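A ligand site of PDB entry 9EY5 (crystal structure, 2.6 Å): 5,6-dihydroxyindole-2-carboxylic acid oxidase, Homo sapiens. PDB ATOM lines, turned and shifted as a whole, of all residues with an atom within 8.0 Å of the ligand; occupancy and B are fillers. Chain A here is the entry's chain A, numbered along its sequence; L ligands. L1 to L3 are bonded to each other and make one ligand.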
ATOM      1  N   THR A 139       5.533 -16.516   7.501  1.00  0.00           N
ATOM      2  CA  THR A 139       6.189 -16.256   6.220  1.00  0.00           C
ATOM      3  C   THR A 139       5.529 -17.015   5.072  1.00  0.00           C
ATOM      4  O   THR A 139       5.871 -16.769   3.913  1.00  0.00           O
ATOM      5  CB  THR A 139       7.666 -16.606   6.298  1.00  0.00           C
ATOM      6  OG1 THR A 139       7.822 -18.023   6.374  1.00  0.00           O
ATOM      7  CG2 THR A 139       8.297 -15.987   7.547  1.00  0.00           C
ATOM      8  N   ARG A 140       4.577 -17.912   5.379  1.00  0.00           N
ATOM      9  CA  ARG A 140       3.868 -18.681   4.376  1.00  0.00           C
ATOM     10  C   ARG A 140       2.361 -18.542   4.580  1.00  0.00           C
ATOM     11  O   ARG A 140       1.892 -18.340   5.696  1.00  0.00           O
ATOM     12  CB  ARG A 140       4.273 -20.150   4.423  1.00  0.00           C
ATOM     13  CG  ARG A 140       5.757 -20.349   4.224  1.00  0.00           C
ATOM     14  CD  ARG A 140       6.162 -19.972   2.813  1.00  0.00           C
ATOM     15  NE  ARG A 140       7.581 -20.235   2.578  1.00  0.00           N
ATOM     16  CZ  ARG A 140       8.552 -19.331   2.701  1.00  0.00           C
ATOM     17  NH1 ARG A 140       8.305 -18.086   3.059  1.00  0.00           N
ATOM     18  NH2 ARG A 140       9.805 -19.696   2.450  1.00  0.00           N
ATOM     19  N   GLN A 154       5.996 -22.177   9.915  1.00  0.00           N
ATOM     20  CA  GLN A 154       6.694 -21.133   9.141  1.00  0.00           C
ATOM     21  C   GLN A 154       6.448 -19.756   9.778  1.00  0.00           C
ATOM     22  O   GLN A 154       5.816 -18.859   9.214  1.00  0.00           O
ATOM     23  CB  GLN A 154       6.249 -21.142   7.691  1.00  0.00           C
ATOM     24  CG  GLN A 154       6.383 -22.486   7.042  1.00  0.00           C
ATOM     25  CD  GLN A 154       7.822 -22.906   6.889  1.00  0.00           C
ATOM     26  OE1 GLN A 154       8.540 -22.360   6.049  1.00  0.00           O
ATOM     27  NE2 GLN A 154       8.249 -23.882   7.685  1.00  0.00           N
ATOM     28  N   GLU A 156       8.418 -16.502  12.025  1.00  0.00           N
ATOM     29  CA  GLU A 156       9.673 -15.827  12.291  1.00  0.00           C
ATOM     30  C   GLU A 156       9.509 -14.831  13.433  1.00  0.00           C
ATOM     31  O   GLU A 156       8.444 -14.229  13.607  1.00  0.00           O
ATOM     32  CB  GLU A 156      10.177 -15.090  11.047  1.00  0.00           C
ATOM     33  CG  GLU A 156      11.368 -15.772  10.402  1.00  0.00           C
ATOM     34  CD  GLU A 156      11.511 -15.450   8.941  1.00  0.00           C
ATOM     35  OE1 GLU A 156      11.449 -14.247   8.560  1.00  0.00           O
ATOM     36  OE2 GLU A 156      11.696 -16.428   8.172  1.00  0.00           O
ATOM     37  N   CYS A 266       9.423  -6.129   3.647  1.00  0.00           N
ATOM     38  CA  CYS A 266       8.274  -6.364   2.754  1.00  0.00           C
ATOM     39  C   CYS A 266       8.449  -5.746   1.357  1.00  0.00           C
ATOM     40  O   CYS A 266       7.463  -5.498   0.660  1.00  0.00           O
ATOM     41  CB  CYS A 266       6.961  -5.873   3.374  1.00  0.00           C
ATOM     42  SG  CYS A 266       6.658  -6.517   5.066  1.00  0.00           S
ATOM     43  N   ASP A 267       9.687  -5.522   0.912  1.00  0.00           N
ATOM     44  CA  ASP A 267       9.928  -4.961  -0.423  1.00  0.00           C
ATOM     45  C   ASP A 267      10.336  -6.059  -1.417  1.00  0.00           C
ATOM     46  O   ASP A 267      11.437  -6.064  -1.982  1.00  0.00           O
ATOM     47  CB  ASP A 267      10.981  -3.859  -0.361  1.00  0.00           C
ATOM     48  CG  ASP A 267      10.988  -2.979  -1.615  1.00  0.00           C
ATOM     49  OD1 ASP A 267      10.003  -3.030  -2.385  1.00  0.00           O
ATOM     50  OD2 ASP A 267      11.982  -2.243  -1.816  1.00  0.00           O
ATOM     51  N   SER A 268       9.433  -7.012  -1.629  1.00  0.00           N
ATOM     52  CA  SER A 268       9.628  -8.102  -2.570  1.00  0.00           C
ATOM     53  C   SER A 268       8.297  -8.528  -3.188  1.00  0.00           C
ATOM     54  O   SER A 268       8.043  -9.713  -3.383  1.00  0.00           O
ATOM     55  CB  SER A 268      10.296  -9.322  -1.912  1.00  0.00           C
ATOM     56  OG  SER A 268      11.618  -9.081  -1.505  1.00  0.00           O
ATOM     57  N   LEU A 269       7.433  -7.543  -3.499  1.00  0.00           N
ATOM     58  CA  LEU A 269       6.134  -7.863  -4.091  1.00  0.00           C
ATOM     59  C   LEU A 269       6.247  -8.881  -5.212  1.00  0.00           C
ATOM     60  O   LEU A 269       5.413  -9.778  -5.338  1.00  0.00           O
ATOM     61  CB  LEU A 269       5.455  -6.594  -4.612  1.00  0.00           C
ATOM     62  CG  LEU A 269       4.874  -5.606  -3.603  1.00  0.00           C
ATOM     63  CD1 LEU A 269       3.965  -4.630  -4.297  1.00  0.00           C
ATOM     64  CD2 LEU A 269       4.141  -6.300  -2.465  1.00  0.00           C
ATOM     65  N   GLU A 270       7.305  -8.781  -6.018  1.00  0.00           N
ATOM     66  CA  GLU A 270       7.499  -9.721  -7.125  1.00  0.00           C
ATOM     67  C   GLU A 270       7.720 -11.134  -6.591  1.00  0.00           C
ATOM     68  O   GLU A 270       7.136 -12.093  -7.101  1.00  0.00           O
ATOM     69  CB  GLU A 270       8.671  -9.266  -7.991  1.00  0.00           C
ATOM     70  CG  GLU A 270       8.878 -10.058  -9.281  1.00  0.00           C
ATOM     71  CD  GLU A 270      10.082  -9.561 -10.091  1.00  0.00           C
ATOM     72  OE1 GLU A 270      10.764  -8.602  -9.650  1.00  0.00           O
ATOM     73  OE2 GLU A 270      10.342 -10.131 -11.175  1.00  0.00           O
ATOM     74  N   ASP A 271       8.544 -11.272  -5.557  1.00  0.00           N
ATOM     75  CA  ASP A 271       8.768 -12.591  -4.957  1.00  0.00           C
ATOM     76  C   ASP A 271       7.467 -13.143  -4.380  1.00  0.00           C
ATOM     77  O   ASP A 271       7.089 -14.289  -4.656  1.00  0.00           O
ATOM     78  CB  ASP A 271       9.859 -12.503  -3.894  1.00  0.00           C
ATOM     79  CG  ASP A 271      11.239 -12.771  -4.455  1.00  0.00           C
ATOM     80  OD1 ASP A 271      11.331 -12.835  -5.691  1.00  0.00           O
ATOM     81  OD2 ASP A 271      12.211 -12.924  -3.688  1.00  0.00           O
ATOM     82  N   TYR A 272       6.768 -12.347  -3.562  1.00  0.00           N
ATOM     83  CA  TYR A 272       5.573 -12.847  -2.891  1.00  0.00           C
ATOM     84  C   TYR A 272       4.500 -13.225  -3.906  1.00  0.00           C
ATOM     85  O   TYR A 272       3.969 -14.341  -3.884  1.00  0.00           O
ATOM     86  CB  TYR A 272       5.033 -11.808  -1.906  1.00  0.00           C
ATOM     87  CG  TYR A 272       6.085 -11.159  -1.028  1.00  0.00           C
ATOM     88  CD1 TYR A 272       7.087 -11.917  -0.417  1.00  0.00           C
ATOM     89  CD2 TYR A 272       6.073  -9.780  -0.802  1.00  0.00           C
ATOM     90  CE1 TYR A 272       8.043 -11.319   0.387  1.00  0.00           C
ATOM     91  CE2 TYR A 272       7.025  -9.173   0.004  1.00  0.00           C
ATOM     92  CZ  TYR A 272       8.009  -9.935   0.589  1.00  0.00           C
ATOM     93  OH  TYR A 272       8.956  -9.338   1.373  1.00  0.00           O
ATOM     94  N   THR A 274       4.554 -14.180  -6.807  1.00  0.00           N
ATOM     95  CA  THR A 274       4.820 -15.329  -7.658  1.00  0.00           C
ATOM     96  C   THR A 274       5.228 -16.569  -6.875  1.00  0.00           C
ATOM     97  O   THR A 274       4.634 -17.629  -7.082  1.00  0.00           O
ATOM     98  CB  THR A 274       5.902 -14.989  -8.721  1.00  0.00           C
ATOM     99  OG1 THR A 274       7.210 -15.042  -8.158  1.00  0.00           O
ATOM    100  CG2 THR A 274       5.652 -13.613  -9.332  1.00  0.00           C
ATOM    101  N   LEU A 275       6.190 -16.471  -5.938  1.00  0.00           N
ATOM    102  CA  LEU A 275       6.544 -17.630  -5.131  1.00  0.00           C
ATOM    103  C   LEU A 275       5.395 -18.102  -4.234  1.00  0.00           C
ATOM    104  O   LEU A 275       5.460 -19.226  -3.717  1.00  0.00           O
ATOM    105  CB  LEU A 275       7.773 -17.356  -4.270  1.00  0.00           C
ATOM    106  CG  LEU A 275       9.149 -17.666  -4.856  1.00  0.00           C
ATOM    107  CD1 LEU A 275      10.156 -17.928  -3.738  1.00  0.00           C
ATOM    108  CD2 LEU A 275       9.065 -18.855  -5.790  1.00  0.00           C
ATOM    109  N   THR A 277       4.648 -16.627  -1.336  1.00  0.00           N
ATOM    110  CA  THR A 277       5.122 -16.445   0.030  1.00  0.00           C
ATOM    111  C   THR A 277       4.633 -15.127   0.627  1.00  0.00           C
ATOM    112  O   THR A 277       3.935 -14.332  -0.021  1.00  0.00           O
ATOM    113  CB  THR A 277       6.648 -16.538   0.058  1.00  0.00           C
ATOM    114  OG1 THR A 277       7.190 -15.547  -0.829  1.00  0.00           O
ATOM    115  CG2 THR A 277       7.092 -17.913  -0.377  1.00  0.00           C
ATOM    116  N   LEU A 278       4.980 -14.892   1.893  1.00  0.00           N
ATOM    117  CA  LEU A 278       4.642 -13.677   2.618  1.00  0.00           C
ATOM    118  C   LEU A 278       5.911 -12.915   3.005  1.00  0.00           C
ATOM    119  O   LEU A 278       6.995 -13.497   3.140  1.00  0.00           O
ATOM    120  CB  LEU A 278       3.826 -13.990   3.887  1.00  0.00           C
ATOM    121  CG  LEU A 278       2.519 -14.769   3.766  1.00  0.00           C
ATOM    122  CD1 LEU A 278       1.813 -14.815   5.119  1.00  0.00           C
ATOM    123  CD2 LEU A 278       1.606 -14.144   2.722  1.00  0.00           C
ATOM    124  N   CYS A 279       5.750 -11.613   3.201  1.00  0.00           N
ATOM    125  CA  CYS A 279       6.846 -10.802   3.739  1.00  0.00           C
ATOM    126  C   CYS A 279       7.371 -11.414   5.029  1.00  0.00           C
ATOM    127  O   CYS A 279       6.607 -11.849   5.887  1.00  0.00           O
ATOM    128  CB  CYS A 279       6.376  -9.363   4.012  1.00  0.00           C
ATOM    129  SG  CYS A 279       7.505  -8.376   5.045  1.00  0.00           S
ATOM    130  N   ASN A 280       8.696 -11.440   5.151  1.00  0.00           N
ATOM    131  CA  ASN A 280       9.368 -11.992   6.318  1.00  0.00           C
ATOM    132  C   ASN A 280      10.177 -10.897   7.016  1.00  0.00           C
ATOM    133  O   ASN A 280      10.048  -9.701   6.719  1.00  0.00           O
ATOM    134  CB  ASN A 280      10.243 -13.179   5.915  1.00  0.00           C
ATOM    135  CG  ASN A 280      11.356 -12.746   5.000  1.00  0.00           C
ATOM    136  OD1 ASN A 280      11.104 -12.156   3.947  1.00  0.00           O
ATOM    137  ND2 ASN A 280      12.596 -12.996   5.427  1.00  0.00           N
ATOM    138  N   SER A 281      11.022 -11.298   7.971  1.00  0.00           N
ATOM    139  CA  SER A 281      11.692 -10.337   8.833  1.00  0.00           C
ATOM    140  C   SER A 281      13.056  -9.923   8.311  1.00  0.00           C
ATOM    141  O   SER A 281      13.745  -9.148   8.993  1.00  0.00           O
ATOM    142  CB  SER A 281      11.844 -10.904  10.254  1.00  0.00           C
ATOM    143  OG  SER A 281      12.601 -12.103  10.225  1.00  0.00           O
ATOM    144  N   THR A 282      13.446 -10.401   7.125  1.00  0.00           N
ATOM    145  CA  THR A 282      14.752 -10.048   6.571  1.00  0.00           C
ATOM    146  C   THR A 282      14.656  -8.686   5.880  1.00  0.00           C
ATOM    147  O   THR A 282      13.854  -8.521   4.952  1.00  0.00           O
ATOM    148  CB  THR A 282      15.218 -11.129   5.596  1.00  0.00           C
ATOM    149  OG1 THR A 282      15.280 -12.380   6.275  1.00  0.00           O
ATOM    150  CG2 THR A 282      16.609 -10.798   5.097  1.00  0.00           C
ATOM    151  N   GLU A 283      15.452  -7.723   6.329  1.00  0.00           N
ATOM    152  CA  GLU A 283      15.411  -6.381   5.777  1.00  0.00           C
ATOM    153  C   GLU A 283      16.256  -6.273   4.505  1.00  0.00           C
ATOM    154  O   GLU A 283      17.142  -7.097   4.243  1.00  0.00           O
ATOM    155  CB  GLU A 283      15.874  -5.376   6.834  1.00  0.00           C
ATOM    156  CG  GLU A 283      15.156  -5.544   8.178  1.00  0.00           C
ATOM    157  CD  GLU A 283      15.755  -4.679   9.268  1.00  0.00           C
ATOM    158  OE1 GLU A 283      16.904  -4.219   9.078  1.00  0.00           O
ATOM    159  OE2 GLU A 283      15.079  -4.462  10.316  1.00  0.00           O
ATOM    160  N   ASP A 284      15.978  -5.232   3.694  1.00  0.00           N
ATOM    161  CA  ASP A 284      16.714  -5.061   2.441  1.00  0.00           C
ATOM    162  C   ASP A 284      16.565  -3.681   1.804  1.00  0.00           C
ATOM    163  O   ASP A 284      15.683  -3.441   0.971  1.00  0.00           O
ATOM    164  CB  ASP A 284      16.266  -6.111   1.421  1.00  0.00           C
ATOM    165  CG  ASP A 284      16.789  -5.827  -0.006  1.00  0.00           C
ATOM    166  OD1 ASP A 284      18.001  -5.466  -0.160  1.00  0.00           O
ATOM    167  OD2 ASP A 284      15.980  -5.964  -0.961  1.00  0.00           O
HETATM  168  C1  LIG L   1      13.156 -13.775   2.715  1.00  0.00           C
HETATM  169  C2  LIG L   1      12.980 -15.212   2.302  1.00  0.00           C
HETATM  170  C3  LIG L   1      13.858 -15.310   1.055  1.00  0.00           C
HETATM  171  C4  LIG L   1      13.599 -14.156   0.071  1.00  0.00           C
HETATM  172  C5  LIG L   1      13.254 -12.804   0.724  1.00  0.00           C
HETATM  173  C6  LIG L   1      12.661 -11.705  -0.161  1.00  0.00           C
HETATM  174  C7  LIG L   1      12.621 -17.133   3.768  1.00  0.00           C
HETATM  175  C8  LIG L   1      13.125 -17.900   4.961  1.00  0.00           C
HETATM  176  N1  LIG L   1      13.336 -16.049   3.428  1.00  0.00           N
HETATM  177  O1  LIG L   1      13.668 -16.567   0.459  1.00  0.00           O
HETATM  178  O2  LIG L   1      14.845 -14.037  -0.530  1.00  0.00           O
HETATM  179  O3  LIG L   1      12.422 -12.999   1.826  1.00  0.00           O
HETATM  180  O4  LIG L   1      11.662 -12.188  -1.019  1.00  0.00           O
HETATM  181  O5  LIG L   1      11.623 -17.491   3.160  1.00  0.00           O
HETATM  182  C1  LG2 L   2      14.817 -14.216  -1.943  1.00  0.00           C
HETATM  183  C2  LG2 L   2      16.298 -14.176  -2.299  1.00  0.00           C
HETATM  184  C3  LG2 L   2      16.469 -14.210  -3.821  1.00  0.00           C
HETATM  185  C4  LG2 L   2      15.762 -15.476  -4.366  1.00  0.00           C
HETATM  186  C5  LG2 L   2      14.361 -15.720  -3.748  1.00  0.00           C
HETATM  187  C6  LG2 L   2      13.903 -17.162  -3.872  1.00  0.00           C
HETATM  188  C7  LG2 L   2      16.627 -11.775  -1.628  1.00  0.00           C
HETATM  189  C8  LG2 L   2      17.436 -10.930  -0.664  1.00  0.00           C
HETATM  190  N1  LG2 L   2      16.909 -13.097  -1.551  1.00  0.00           N
HETATM  191  O1  LG2 L   2      17.846 -14.218  -4.112  1.00  0.00           O
HETATM  192  O2  LG2 L   2      15.677 -15.360  -5.784  1.00  0.00           O
HETATM  193  O3  LG2 L   2      14.265 -15.433  -2.353  1.00  0.00           O
HETATM  194  O4  LG2 L   2      14.395 -17.897  -2.761  1.00  0.00           O
HETATM  195  O5  LG2 L   2      15.801 -11.294  -2.398  1.00  0.00           O
HETATM  196  C1  LG3 L   3      16.622 -16.227  -6.487  1.00  0.00           C
HETATM  197  C2  LG3 L   3      15.927 -16.625  -7.797  1.00  0.00           C
HETATM  198  C3  LG3 L   3      16.896 -17.130  -8.912  1.00  0.00           C
HETATM  199  C4  LG3 L   3      18.313 -16.490  -8.954  1.00  0.00           C
HETATM  200  C5  LG3 L   3      18.843 -15.933  -7.620  1.00  0.00           C
HETATM  201  C6  LG3 L   3      19.858 -14.786  -7.778  1.00  0.00           C
HETATM  202  O1  LG3 L   3      15.096 -15.572  -8.245  1.00  0.00           O
HETATM  203  O2  LG3 L   3      16.162 -17.014 -10.109  1.00  0.00           O
HETATM  204  O3  LG3 L   3      19.172 -17.503  -9.453  1.00  0.00           O
HETATM  205  O4  LG3 L   3      17.863 -15.555  -6.660  1.00  0.00           O
HETATM  206  O5  LG3 L   3      20.792 -14.867  -6.723  1.00  0.00           O
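The side-chain amide oxygen (OD1) of Asn 280 lies close to an oxygen (O3) of LIG L1 (2.6 Å).
The side-chain carboxylate (OD2) of Asp 271 lies within hydrogen-bond range of an oxygen (O4) of LIG L1 (2.8 Å).
O5 of LIG L1 lies within hydrogen-bond range of NH2 of Arg 140 (2.9 Å).
The side-chain hydroxyl of Ser 268 sits close to an oxygen (O4) of LIG L1 (3.1 Å).
The side-chain hydroxyl (OG1) of Thr 282 is in hydrogen-bond range of the side-chain amide nitrogen (ND2) of Asn 280 (2.9 Å).
The guanidinium group (NH1) of Arg 140 sits at hydrogen-bond distance from the side-chain hydroxyl (OG1) of Thr 139.
The side-chain carboxylate (OE1) of Glu 156 lies within hydrogen-bond range of the side-chain hydroxyl (OG) of Ser 281 (2.9 Å).
O of Tyr 272 is in hydrogen-bond range of N of Thr 277.
The side-chain sulfur of Cys 266 is disulfide-bonded to the side-chain sulfur of Cys 279 (2.0 Å).
Residues that only touch the ligand: Glu 156, Leu 275 and Tyr 272.
Seven residues have an atom within 4 Å of the ligand: Arg 140, Glu 156, Ser 268, Asp 271, Tyr 272, Leu 275 and Asn 280.
The nearest printed residue that does not touch the ligand is Thr 282 (4.4 Å).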
